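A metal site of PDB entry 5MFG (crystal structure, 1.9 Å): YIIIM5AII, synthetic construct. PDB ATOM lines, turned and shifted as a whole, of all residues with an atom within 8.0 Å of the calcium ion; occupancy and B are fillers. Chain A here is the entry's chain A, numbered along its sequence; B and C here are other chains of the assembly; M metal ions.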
ATOM      1  N   SER A 225      -8.577  -3.491 -14.552  1.00  0.00           N
ATOM      2  CA  SER A 225      -8.985  -3.402 -13.161  1.00  0.00           C
ATOM      3  C   SER A 225      -8.180  -2.323 -12.445  1.00  0.00           C
ATOM      4  O   SER A 225      -6.972  -2.197 -12.668  1.00  0.00           O
ATOM      5  CB  SER A 225      -8.786  -4.747 -12.464  1.00  0.00           C
ATOM      6  OG  SER A 225      -9.032  -4.646 -11.076  1.00  0.00           O
ATOM      7  N   PRO A 226      -8.812  -1.520 -11.584  1.00  0.00           N
ATOM      8  CA  PRO A 226      -8.055  -0.604 -10.727  1.00  0.00           C
ATOM      9  C   PRO A 226      -7.445  -1.267  -9.511  1.00  0.00           C
ATOM     10  O   PRO A 226      -6.811  -0.582  -8.693  1.00  0.00           O
ATOM     11  CB  PRO A 226      -9.109   0.419 -10.316  1.00  0.00           C
ATOM     12  CG  PRO A 226     -10.368  -0.356 -10.281  1.00  0.00           C
ATOM     13  CD  PRO A 226     -10.263  -1.389 -11.380  1.00  0.00           C
ATOM     14  N   ASN A 227      -7.633  -2.577  -9.360  1.00  0.00           N
ATOM     15  CA  ASN A 227      -7.058  -3.336  -8.250  1.00  0.00           C
ATOM     16  C   ASN A 227      -5.669  -3.806  -8.659  1.00  0.00           C
ATOM     17  O   ASN A 227      -5.529  -4.681  -9.521  1.00  0.00           O
ATOM     18  CB  ASN A 227      -7.962  -4.509  -7.906  1.00  0.00           C
ATOM     19  CG  ASN A 227      -7.430  -5.344  -6.752  1.00  0.00           C
ATOM     20  OD1 ASN A 227      -6.213  -5.484  -6.579  1.00  0.00           O
ATOM     21  ND2 ASN A 227      -8.328  -5.893  -5.962  1.00  0.00           N
ATOM     22  N   GLU A 228      -4.636  -3.224  -8.029  1.00  0.00           N
ATOM     23  CA  GLU A 228      -3.269  -3.556  -8.409  1.00  0.00           C
ATOM     24  C   GLU A 228      -2.930  -5.013  -8.125  1.00  0.00           C
ATOM     25  O   GLU A 228      -2.056  -5.587  -8.775  1.00  0.00           O
ATOM     26  CB  GLU A 228      -2.286  -2.632  -7.683  1.00  0.00           C
ATOM     27  CG  GLU A 228      -2.357  -1.175  -8.119  1.00  0.00           C
ATOM     28  CD  GLU A 228      -3.485  -0.418  -7.446  1.00  0.00           C
ATOM     29  OE1 GLU A 228      -3.310   0.786  -7.164  1.00  0.00           O
ATOM     30  OE2 GLU A 228      -4.555  -1.018  -7.199  1.00  0.00           O
ATOM     31  N   GLN A 229      -3.610  -5.619  -7.147  1.00  0.00           N
ATOM     32  CA  GLN A 229      -3.343  -7.011  -6.821  1.00  0.00           C
ATOM     33  C   GLN A 229      -3.867  -7.932  -7.921  1.00  0.00           C
ATOM     34  O   GLN A 229      -3.174  -8.847  -8.371  1.00  0.00           O
ATOM     35  CB  GLN A 229      -3.976  -7.349  -5.474  1.00  0.00           C
ATOM     36  CG  GLN A 229      -3.323  -8.487  -4.720  1.00  0.00           C
ATOM     37  CD  GLN A 229      -3.723  -8.526  -3.259  1.00  0.00           C
ATOM     38  OE1 GLN A 229      -4.520  -7.707  -2.798  1.00  0.00           O
ATOM     39  NE2 GLN A 229      -3.172  -9.479  -2.517  1.00  0.00           N
ATOM     40  N   SER B 225      -3.758   2.969   2.062  1.00  0.00           N
ATOM     41  CA  SER B 225      -3.487   3.027   0.642  1.00  0.00           C
ATOM     42  C   SER B 225      -4.664   2.471  -0.147  1.00  0.00           C
ATOM     43  O   SER B 225      -5.262   1.464   0.243  1.00  0.00           O
ATOM     44  CB  SER B 225      -2.223   2.222   0.312  1.00  0.00           C
ATOM     45  OG  SER B 225      -2.061   2.086  -1.083  1.00  0.00           O
ATOM     46  N   PRO B 226      -5.031   3.095  -1.272  1.00  0.00           N
ATOM     47  CA  PRO B 226      -5.983   2.472  -2.189  1.00  0.00           C
ATOM     48  C   PRO B 226      -5.363   1.408  -3.082  1.00  0.00           C
ATOM     49  O   PRO B 226      -6.086   0.779  -3.862  1.00  0.00           O
ATOM     50  CB  PRO B 226      -6.465   3.668  -3.029  1.00  0.00           C
ATOM     51  CG  PRO B 226      -5.290   4.560  -3.070  1.00  0.00           C
ATOM     52  CD  PRO B 226      -4.590   4.419  -1.744  1.00  0.00           C
ATOM     53  N   ASN B 227      -4.057   1.206  -2.988  1.00  0.00           N
ATOM     54  CA  ASN B 227      -3.363   0.191  -3.752  1.00  0.00           C
ATOM     55  C   ASN B 227      -3.463  -1.122  -2.973  1.00  0.00           C
ATOM     56  O   ASN B 227      -2.877  -1.260  -1.900  1.00  0.00           O
ATOM     57  CB  ASN B 227      -1.914   0.603  -3.972  1.00  0.00           C
ATOM     58  CG  ASN B 227      -1.126  -0.410  -4.766  1.00  0.00           C
ATOM     59  OD1 ASN B 227      -1.414  -1.606  -4.747  1.00  0.00           O
ATOM     60  ND2 ASN B 227      -0.103   0.062  -5.461  1.00  0.00           N
ATOM     61  N   GLU B 228      -4.204  -2.075  -3.525  1.00  0.00           N
ATOM     62  CA  GLU B 228      -4.405  -3.344  -2.834  1.00  0.00           C
ATOM     63  C   GLU B 228      -3.119  -4.160  -2.777  1.00  0.00           C
ATOM     64  O   GLU B 228      -2.964  -5.002  -1.877  1.00  0.00           O
ATOM     65  CB  GLU B 228      -5.501  -4.157  -3.519  1.00  0.00           C
ATOM     66  CG  GLU B 228      -6.872  -3.511  -3.454  1.00  0.00           C
ATOM     67  CD  GLU B 228      -7.073  -2.424  -4.490  1.00  0.00           C
ATOM     68  OE1 GLU B 228      -8.239  -2.188  -4.892  1.00  0.00           O
ATOM     69  OE2 GLU B 228      -6.073  -1.803  -4.920  1.00  0.00           O
ATOM     70  N   GLN B 229      -2.184  -3.931  -3.698  1.00  0.00           N
ATOM     71  CA  GLN B 229      -0.897  -4.617  -3.657  1.00  0.00           C
ATOM     72  C   GLN B 229      -0.082  -4.151  -2.456  1.00  0.00           C
ATOM     73  O   GLN B 229       0.449  -4.967  -1.694  1.00  0.00           O
ATOM     74  CB  GLN B 229      -0.150  -4.380  -4.962  1.00  0.00           C
ATOM     75  CG  GLN B 229       0.842  -5.455  -5.334  1.00  0.00           C
ATOM     76  CD  GLN B 229       1.248  -5.380  -6.795  1.00  0.00           C
ATOM     77  OE1 GLN B 229       0.989  -4.386  -7.480  1.00  0.00           O
ATOM     78  NE2 GLN B 229       1.872  -6.449  -7.285  1.00  0.00           N
ATOM     79  N   ILE C  62      -8.841  -8.633   0.663  1.00  0.00           N
ATOM     80  CA  ILE C  62      -8.476  -7.677   1.703  1.00  0.00           C
ATOM     81  C   ILE C  62      -9.006  -8.146   3.050  1.00  0.00           C
ATOM     82  O   ILE C  62      -8.326  -8.022   4.080  1.00  0.00           O
ATOM     83  CB  ILE C  62      -9.022  -6.272   1.352  1.00  0.00           C
ATOM     84  CG1 ILE C  62      -8.340  -5.737   0.099  1.00  0.00           C
ATOM     85  CG2 ILE C  62      -8.836  -5.327   2.524  1.00  0.00           C
ATOM     86  CD1 ILE C  62      -9.010  -4.502  -0.468  1.00  0.00           C
HETATM   87 CA    CA M   1      -6.626   0.390  -6.133  1.00  0.00          CA
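The backbone carbonyl oxygen of Glu 228 of chain B lies close to the side-chain amide oxygen of Gln 229 of chain A.
The nearest printed residue that does not touch the calcium ion is Asn 227 of chain B (4.04 Å).
The calcium ion is bound by O of Pro 226 of chain B (2.4 Å), OE2 of Glu 228 of chain B (2.6 Å), OE2 of Glu 228 of chain A (2.7 Å) and O of Pro 226 of chain A (2.7 Å).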
